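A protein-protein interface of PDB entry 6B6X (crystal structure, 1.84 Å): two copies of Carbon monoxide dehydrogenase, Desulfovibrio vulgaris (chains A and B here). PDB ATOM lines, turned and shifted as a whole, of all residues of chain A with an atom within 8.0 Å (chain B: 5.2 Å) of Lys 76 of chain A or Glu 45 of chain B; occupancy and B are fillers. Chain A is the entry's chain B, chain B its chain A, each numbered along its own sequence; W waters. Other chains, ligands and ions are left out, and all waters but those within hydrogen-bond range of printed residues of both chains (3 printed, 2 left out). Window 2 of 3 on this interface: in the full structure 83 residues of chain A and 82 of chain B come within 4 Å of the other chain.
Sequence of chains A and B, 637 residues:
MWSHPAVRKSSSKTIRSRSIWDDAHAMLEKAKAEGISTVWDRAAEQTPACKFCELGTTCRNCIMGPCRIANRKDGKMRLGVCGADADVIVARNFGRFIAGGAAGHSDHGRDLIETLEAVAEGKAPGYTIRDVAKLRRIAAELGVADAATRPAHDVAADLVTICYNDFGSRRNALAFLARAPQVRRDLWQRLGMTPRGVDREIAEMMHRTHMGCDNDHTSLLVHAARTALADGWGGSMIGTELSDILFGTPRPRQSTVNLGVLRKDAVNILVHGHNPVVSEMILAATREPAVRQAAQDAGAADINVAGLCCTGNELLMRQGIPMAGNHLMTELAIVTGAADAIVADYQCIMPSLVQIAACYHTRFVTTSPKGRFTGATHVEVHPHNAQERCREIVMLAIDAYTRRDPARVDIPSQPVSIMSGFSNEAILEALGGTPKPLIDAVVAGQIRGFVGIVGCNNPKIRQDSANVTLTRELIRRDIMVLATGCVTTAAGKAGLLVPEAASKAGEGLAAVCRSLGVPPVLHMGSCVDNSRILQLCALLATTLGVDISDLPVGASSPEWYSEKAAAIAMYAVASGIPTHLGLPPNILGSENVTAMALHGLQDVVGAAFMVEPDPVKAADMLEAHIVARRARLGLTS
The guanidinium group (NE) of Arg 42 of chain B lies within hydrogen-bond range of the backbone carbonyl oxygen (O) of Gly 80 of chain A (3.4 Å).
O of Val 81 of chain A lies within hydrogen-bond range of NE of Arg 42 of chain B, 2.8 Å away.
The backbone NH (N) of Met 77 of chain A sits at hydrogen-bond distance from the side-chain carboxylate (OE1) of Glu 45 of chain B (3.0 Å).
NE2 of Gln 46 of chain B is in hydrogen-bond range of O of Arg 68 of chain A, 2.9 Å away.
The backbone carbonyl oxygen (O) of Leu 79 of chain A lies within hydrogen-bond range of the side-chain amide nitrogen (NE2) of Gln 46 of chain B (3.1 Å).
OG1 of Thr 47 of chain B sits at hydrogen-bond distance from O of Ala 43 of chain B (2.9 Å).
The backbone carbonyl oxygen of Met 77 of chain A lies within hydrogen-bond range of the backbone NH of Ala 70 of chain A (3.0 Å).
The side-chain carboxylate of Asp 74 of chain A lies close to the backbone NH of Lys 76 of chain A (3.2 Å).
CA of Lys 76 of chain A touches OE1 of Glu 45 of chain B, at 3.6 Å.
Gln 46 of chain B touches Met 77 of chain A.
Ala 43 of chain B touches Val 81 of chain A (CA to CG2, 3.7 Å).
Gln 46 of chain B touches Val 81 of chain A (CG to CG2, 3.9 Å).
Lys 76 of chain A touches just one residue of chain B: Glu 45.
Glu 45 of chain B touches two residues of chain A.
Ala 44 of chain B touches none of the printed residues of chain A.
Of the printed residues of chain B, Met 77 of chain A touches Glu 45 (3.0 Å) and Gln 46 (3.6 Å).
Of the printed residues of chain A, Arg 42 of chain B touches Gly 80 and Val 81.
Of the printed residues of chain B, Gly 80 of chain A touches Arg 42.
The nearest printed residue of chain B that does not touch Lys 76 of chain A is Gln 46 of chain B (6.3 Å).
Of the 7 printed residues of chain B, 4 touch a printed residue of chain A.
Among the printed residues, 9 pairs touch across the chains.
Among the printed residues, no Asp or Glu carboxylate lies within 4 Å of a Lys or Arg side-chain nitrogen of the other chain.
No position is printed for both chains.
Of the 9 pairs that touch across the chains among the printed residues, none has its exchanged pair printed and touching as well.
Water W2 bridges the side-chain amide oxygen (OE1) of Gln 46 of chain B (2.6 Å) and the guanidinium group (NH2) of Arg 68 of chain A (3.0 Å).
Water W3 lies within hydrogen-bond range of OE1 of Glu 45 of chain B (2.6 Å) and O of Leu 79 of chain A (2.7 Å).
Water W1 bridges the backbone carbonyl oxygen (O) of Pro 66 of chain A (2.7 Å) and the backbone carbonyl oxygen (O) of Gln 46 of chain B (2.8 Å).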
ATOM      1  N   PRO A  66     -31.451 -31.586 -11.247  1.00  0.00           N
ATOM      2  CA  PRO A  66     -31.635 -30.131 -11.185  1.00  0.00           C
ATOM      3  C   PRO A  66     -30.558 -29.402 -10.382  1.00  0.00           C
ATOM      4  O   PRO A  66     -29.868 -30.012  -9.558  1.00  0.00           O
ATOM      5  CB  PRO A  66     -33.002 -29.990 -10.507  1.00  0.00           C
ATOM      6  CG  PRO A  66     -33.100 -31.182  -9.633  1.00  0.00           C
ATOM      7  CD  PRO A  66     -32.430 -32.298 -10.406  1.00  0.00           C
ATOM      8  N   ARG A  68     -29.204 -25.659  -8.298  1.00  0.00           N
ATOM      9  CA  ARG A  68     -29.486 -24.425  -7.581  1.00  0.00           C
ATOM     10  C   ARG A  68     -28.201 -23.620  -7.490  1.00  0.00           C
ATOM     11  O   ARG A  68     -27.117 -24.186  -7.322  1.00  0.00           O
ATOM     12  CB  ARG A  68     -30.025 -24.698  -6.173  1.00  0.00           C
ATOM     13  CG  ARG A  68     -31.469 -25.195  -6.129  1.00  0.00           C
ATOM     14  CD  ARG A  68     -31.737 -25.879  -4.799  1.00  0.00           C
ATOM     15  NE  ARG A  68     -30.981 -27.119  -4.688  1.00  0.00           N
ATOM     16  CZ  ARG A  68     -30.526 -27.622  -3.544  1.00  0.00           C
ATOM     17  NH1 ARG A  68     -30.752 -26.987  -2.402  1.00  0.00           N
ATOM     18  NH2 ARG A  68     -29.838 -28.755  -3.544  1.00  0.00           N
ATOM     19  N   ILE A  69     -28.319 -22.302  -7.607  1.00  0.00           N
ATOM     20  CA  ILE A  69     -27.174 -21.405  -7.501  1.00  0.00           C
ATOM     21  C   ILE A  69     -27.246 -20.719  -6.148  1.00  0.00           C
ATOM     22  O   ILE A  69     -28.234 -20.043  -5.838  1.00  0.00           O
ATOM     23  CB  ILE A  69     -27.142 -20.376  -8.639  1.00  0.00           C
ATOM     24  CG1 ILE A  69     -27.110 -21.083  -9.992  1.00  0.00           C
ATOM     25  CG2 ILE A  69     -25.937 -19.453  -8.478  1.00  0.00           C
ATOM     26  CD1 ILE A  69     -25.984 -22.097 -10.135  1.00  0.00           C
ATOM     27  N   ALA A  70     -26.207 -20.899  -5.343  1.00  0.00           N
ATOM     28  CA  ALA A  70     -26.141 -20.326  -4.010  1.00  0.00           C
ATOM     29  C   ALA A  70     -24.902 -19.449  -3.886  1.00  0.00           C
ATOM     30  O   ALA A  70     -23.991 -19.492  -4.718  1.00  0.00           O
ATOM     31  CB  ALA A  70     -26.136 -21.425  -2.941  1.00  0.00           C
ATOM     32  N   ASN A  71     -24.884 -18.639  -2.833  1.00  0.00           N
ATOM     33  CA  ASN A  71     -23.747 -17.786  -2.500  1.00  0.00           C
ATOM     34  C   ASN A  71     -23.157 -18.338  -1.204  1.00  0.00           C
ATOM     35  O   ASN A  71     -23.496 -17.891  -0.108  1.00  0.00           O
ATOM     36  CB  ASN A  71     -24.168 -16.326  -2.361  1.00  0.00           C
ATOM     37  CG  ASN A  71     -22.988 -15.375  -2.367  1.00  0.00           C
ATOM     38  OD1 ASN A  71     -21.869 -15.751  -2.020  1.00  0.00           O
ATOM     39  ND2 ASN A  71     -23.234 -14.132  -2.763  1.00  0.00           N
ATOM     40  N   ARG A  72     -22.275 -19.322  -1.339  1.00  0.00           N
ATOM     41  CA  ARG A  72     -21.705 -20.024  -0.203  1.00  0.00           C
ATOM     42  C   ARG A  72     -20.238 -19.649  -0.025  1.00  0.00           C
ATOM     43  O   ARG A  72     -19.539 -19.327  -0.991  1.00  0.00           O
ATOM     44  CB  ARG A  72     -21.844 -21.539  -0.374  1.00  0.00           C
ATOM     45  CG  ARG A  72     -23.286 -22.013  -0.426  1.00  0.00           C
ATOM     46  CD  ARG A  72     -23.375 -23.520  -0.597  1.00  0.00           C
ATOM     47  NE  ARG A  72     -22.603 -24.233   0.417  1.00  0.00           N
ATOM     48  CZ  ARG A  72     -22.733 -25.530   0.678  1.00  0.00           C
ATOM     49  NH1 ARG A  72     -21.986 -26.096   1.617  1.00  0.00           N
ATOM     50  NH2 ARG A  72     -23.614 -26.259   0.009  1.00  0.00           N
ATOM     51  N   LYS A  73     -19.783 -19.696   1.229  1.00  0.00           N
ATOM     52  CA  LYS A  73     -18.412 -19.303   1.537  1.00  0.00           C
ATOM     53  C   LYS A  73     -17.405 -20.251   0.896  1.00  0.00           C
ATOM     54  O   LYS A  73     -16.359 -19.812   0.403  1.00  0.00           O
ATOM     55  CB  LYS A  73     -18.209 -19.243   3.050  1.00  0.00           C
ATOM     56  N   ASP A  74     -17.701 -21.552   0.884  1.00  0.00           N
ATOM     57  CA  ASP A  74     -16.802 -22.510   0.249  1.00  0.00           C
ATOM     58  C   ASP A  74     -16.814 -22.423  -1.273  1.00  0.00           C
ATOM     59  O   ASP A  74     -16.127 -23.217  -1.925  1.00  0.00           O
ATOM     60  CB  ASP A  74     -17.145 -23.936   0.695  1.00  0.00           C
ATOM     61  CG  ASP A  74     -18.588 -24.319   0.411  1.00  0.00           C
ATOM     62  OD1 ASP A  74     -19.316 -23.525  -0.223  1.00  0.00           O
ATOM     63  OD2 ASP A  74     -18.997 -25.423   0.830  1.00  0.00           O
ATOM     64  N   GLY A  75     -17.569 -21.489  -1.851  1.00  0.00           N
ATOM     65  CA  GLY A  75     -17.611 -21.305  -3.287  1.00  0.00           C
ATOM     66  C   GLY A  75     -18.378 -22.355  -4.055  1.00  0.00           C
ATOM     67  O   GLY A  75     -18.421 -22.283  -5.288  1.00  0.00           O
ATOM     68  N   LYS A  76     -18.982 -23.326  -3.378  1.00  0.00           N
ATOM     69  CA  LYS A  76     -19.697 -24.389  -4.063  1.00  0.00           C
ATOM     70  C   LYS A  76     -21.062 -23.905  -4.537  1.00  0.00           C
ATOM     71  O   LYS A  76     -21.623 -22.932  -4.022  1.00  0.00           O
ATOM     72  CB  LYS A  76     -19.864 -25.604  -3.153  1.00  0.00           C
ATOM     73  CG  LYS A  76     -18.557 -26.290  -2.782  1.00  0.00           C
ATOM     74  CD  LYS A  76     -18.810 -27.569  -2.001  1.00  0.00           C
ATOM     75  CE  LYS A  76     -17.502 -28.212  -1.571  1.00  0.00           C
ATOM     76  NZ  LYS A  76     -16.605 -28.452  -2.733  1.00  0.00           N
ATOM     77  N   MET A  77     -21.595 -24.612  -5.538  1.00  0.00           N
ATOM     78  CA  MET A  77     -22.907 -24.329  -6.124  1.00  0.00           C
ATOM     79  C   MET A  77     -22.979 -22.927  -6.721  1.00  0.00           C
ATOM     80  O   MET A  77     -24.053 -22.325  -6.799  1.00  0.00           O
ATOM     81  CB  MET A  77     -24.034 -24.539  -5.107  1.00  0.00           C
ATOM     82  CG  MET A  77     -24.104 -25.953  -4.558  1.00  0.00           C
ATOM     83  SD  MET A  77     -25.446 -26.186  -3.374  1.00  0.00           S
ATOM     84  CE  MET A  77     -26.890 -25.993  -4.420  1.00  0.00           C
ATOM     85  N   ARG A  78     -21.836 -22.399  -7.158  1.00  0.00           N
ATOM     86  CA  ARG A  78     -21.839 -21.180  -7.953  1.00  0.00           C
ATOM     87  C   ARG A  78     -22.292 -21.441  -9.383  1.00  0.00           C
ATOM     88  O   ARG A  78     -22.777 -20.519 -10.049  1.00  0.00           O
ATOM     89  CB  ARG A  78     -20.440 -20.547  -7.950  1.00  0.00           C
ATOM     90  CG  ARG A  78     -20.373 -19.162  -8.587  1.00  0.00           C
ATOM     91  CD  ARG A  78     -18.968 -18.574  -8.517  1.00  0.00           C
ATOM     92  NE  ARG A  78     -17.970 -19.450  -9.126  1.00  0.00           N
ATOM     93  CZ  ARG A  78     -17.618 -19.411 -10.408  1.00  0.00           C
ATOM     94  NH1 ARG A  78     -16.702 -20.251 -10.869  1.00  0.00           N
ATOM     95  NH2 ARG A  78     -18.181 -18.537 -11.229  1.00  0.00           N
ATOM     96  N   LEU A  79     -22.171 -22.681  -9.854  1.00  0.00           N
ATOM     97  CA  LEU A  79     -22.478 -23.039 -11.230  1.00  0.00           C
ATOM     98  C   LEU A  79     -23.321 -24.304 -11.259  1.00  0.00           C
ATOM     99  O   LEU A  79     -23.195 -25.174 -10.391  1.00  0.00           O
ATOM    100  CB  LEU A  79     -21.193 -23.267 -12.048  1.00  0.00           C
ATOM    101  CG  LEU A  79     -20.157 -22.143 -12.064  1.00  0.00           C
ATOM    102  CD1 LEU A  79     -18.871 -22.599 -12.747  1.00  0.00           C
ATOM    103  CD2 LEU A  79     -20.728 -20.911 -12.749  1.00  0.00           C
ATOM    104  N   GLY A  80     -24.178 -24.404 -12.271  1.00  0.00           N
ATOM    105  CA  GLY A  80     -24.848 -25.654 -12.553  1.00  0.00           C
ATOM    106  C   GLY A  80     -23.867 -26.708 -13.040  1.00  0.00           C
ATOM    107  O   GLY A  80     -22.694 -26.441 -13.311  1.00  0.00           O
ATOM    108  N   VAL A  81     -24.365 -27.943 -13.149  1.00  0.00           N
ATOM    109  CA  VAL A  81     -23.491 -29.048 -13.536  1.00  0.00           C
ATOM    110  C   VAL A  81     -22.902 -28.797 -14.917  1.00  0.00           C
ATOM    111  O   VAL A  81     -21.733 -29.099 -15.171  1.00  0.00           O
ATOM    112  CB  VAL A  81     -24.248 -30.388 -13.471  1.00  0.00           C
ATOM    113  CG1 VAL A  81     -23.316 -31.541 -13.823  1.00  0.00           C
ATOM    114  CG2 VAL A  81     -24.831 -30.596 -12.084  1.00  0.00           C
ATOM    115  N   ASP B  41     -17.105 -32.647 -11.047  1.00  0.00           N
ATOM    116  CA  ASP B  41     -16.934 -31.890  -9.813  1.00  0.00           C
ATOM    117  C   ASP B  41     -18.169 -31.059  -9.498  1.00  0.00           C
ATOM    118  O   ASP B  41     -18.577 -30.958  -8.336  1.00  0.00           O
ATOM    119  CB  ASP B  41     -15.705 -30.992  -9.912  1.00  0.00           C
ATOM    120  CG  ASP B  41     -14.426 -31.780 -10.089  1.00  0.00           C
ATOM    121  OD1 ASP B  41     -14.223 -32.758  -9.338  1.00  0.00           O
ATOM    122  OD2 ASP B  41     -13.634 -31.429 -10.986  1.00  0.00           O
ATOM    123  N   ARG B  42     -18.776 -30.452 -10.521  1.00  0.00           N
ATOM    124  CA  ARG B  42     -19.967 -29.645 -10.289  1.00  0.00           C
ATOM    125  C   ARG B  42     -21.186 -30.516 -10.005  1.00  0.00           C
ATOM    126  O   ARG B  42     -22.070 -30.109  -9.243  1.00  0.00           O
ATOM    127  CB  ARG B  42     -20.208 -28.728 -11.490  1.00  0.00           C
ATOM    128  CG  ARG B  42     -19.032 -27.793 -11.770  1.00  0.00           C
ATOM    129  CD  ARG B  42     -19.319 -26.825 -12.907  1.00  0.00           C
ATOM    130  NE  ARG B  42     -19.601 -27.512 -14.166  1.00  0.00           N
ATOM    131  CZ  ARG B  42     -18.679 -27.846 -15.065  1.00  0.00           C
ATOM    132  NH1 ARG B  42     -17.399 -27.567 -14.850  1.00  0.00           N
ATOM    133  NH2 ARG B  42     -19.040 -28.467 -16.179  1.00  0.00           N
ATOM    134  N   ALA B  43     -21.253 -31.709 -10.601  1.00  0.00           N
ATOM    135  CA  ALA B  43     -22.313 -32.650 -10.254  1.00  0.00           C
ATOM    136  C   ALA B  43     -22.264 -33.016  -8.774  1.00  0.00           C
ATOM    137  O   ALA B  43     -23.308 -33.134  -8.119  1.00  0.00           O
ATOM    138  CB  ALA B  43     -22.203 -33.905 -11.121  1.00  0.00           C
ATOM    139  N   ALA B  44     -21.058 -33.200  -8.231  1.00  0.00           N
ATOM    140  CA  ALA B  44     -20.925 -33.502  -6.809  1.00  0.00           C
ATOM    141  C   ALA B  44     -21.404 -32.338  -5.948  1.00  0.00           C
ATOM    142  O   ALA B  44     -22.012 -32.548  -4.893  1.00  0.00           O
ATOM    143  CB  ALA B  44     -19.472 -33.856  -6.479  1.00  0.00           C
ATOM    144  N   GLU B  45     -21.140 -31.101  -6.382  1.00  0.00           N
ATOM    145  CA  GLU B  45     -21.583 -29.942  -5.609  1.00  0.00           C
ATOM    146  C   GLU B  45     -23.101 -29.814  -5.599  1.00  0.00           C
ATOM    147  O   GLU B  45     -23.672 -29.312  -4.625  1.00  0.00           O
ATOM    148  CB  GLU B  45     -20.967 -28.660  -6.166  1.00  0.00           C
ATOM    149  CG  GLU B  45     -19.455 -28.575  -6.069  1.00  0.00           C
ATOM    150  CD  GLU B  45     -18.917 -27.291  -6.670  1.00  0.00           C
ATOM    151  OE1 GLU B  45     -19.732 -26.401  -7.002  1.00  0.00           O
ATOM    152  OE2 GLU B  45     -17.684 -27.172  -6.819  1.00  0.00           O
ATOM    153  N   GLN B  46     -23.766 -30.236  -6.670  1.00  0.00           N
ATOM    154  CA  GLN B  46     -25.217 -30.154  -6.776  1.00  0.00           C
ATOM    155  C   GLN B  46     -25.916 -31.393  -6.227  1.00  0.00           C
ATOM    156  O   GLN B  46     -27.105 -31.595  -6.497  1.00  0.00           O
ATOM    157  CB  GLN B  46     -25.624 -29.921  -8.233  1.00  0.00           C
ATOM    158  CG  GLN B  46     -25.132 -28.590  -8.801  1.00  0.00           C
ATOM    159  CD  GLN B  46     -25.918 -27.405  -8.269  1.00  0.00           C
ATOM    160  OE1 GLN B  46     -26.994 -27.565  -7.687  1.00  0.00           O
ATOM    161  NE2 GLN B  46     -25.384 -26.205  -8.471  1.00  0.00           N
ATOM    162  N   THR B  47     -25.203 -32.225  -5.473  1.00  0.00           N
ATOM    163  CA  THR B  47     -25.758 -33.394  -4.812  1.00  0.00           C
ATOM    164  C   THR B  47     -25.682 -33.196  -3.309  1.00  0.00           C
ATOM    165  O   THR B  47     -24.597 -32.890  -2.796  1.00  0.00           O
ATOM    166  CB  THR B  47     -24.989 -34.662  -5.212  1.00  0.00           C
ATOM    167  OG1 THR B  47     -25.084 -34.853  -6.629  1.00  0.00           O
ATOM    168  CG2 THR B  47     -25.552 -35.884  -4.502  1.00  0.00           C
HETATM  169  O   HOH W   1     -28.558 -32.229  -8.781  1.00  0.00           O
HETATM  170  O   HOH W   2     -28.526 -29.162  -6.265  1.00  0.00           O
HETATM  171  O   HOH W   3     -21.865 -26.600  -8.558  1.00  0.00           O
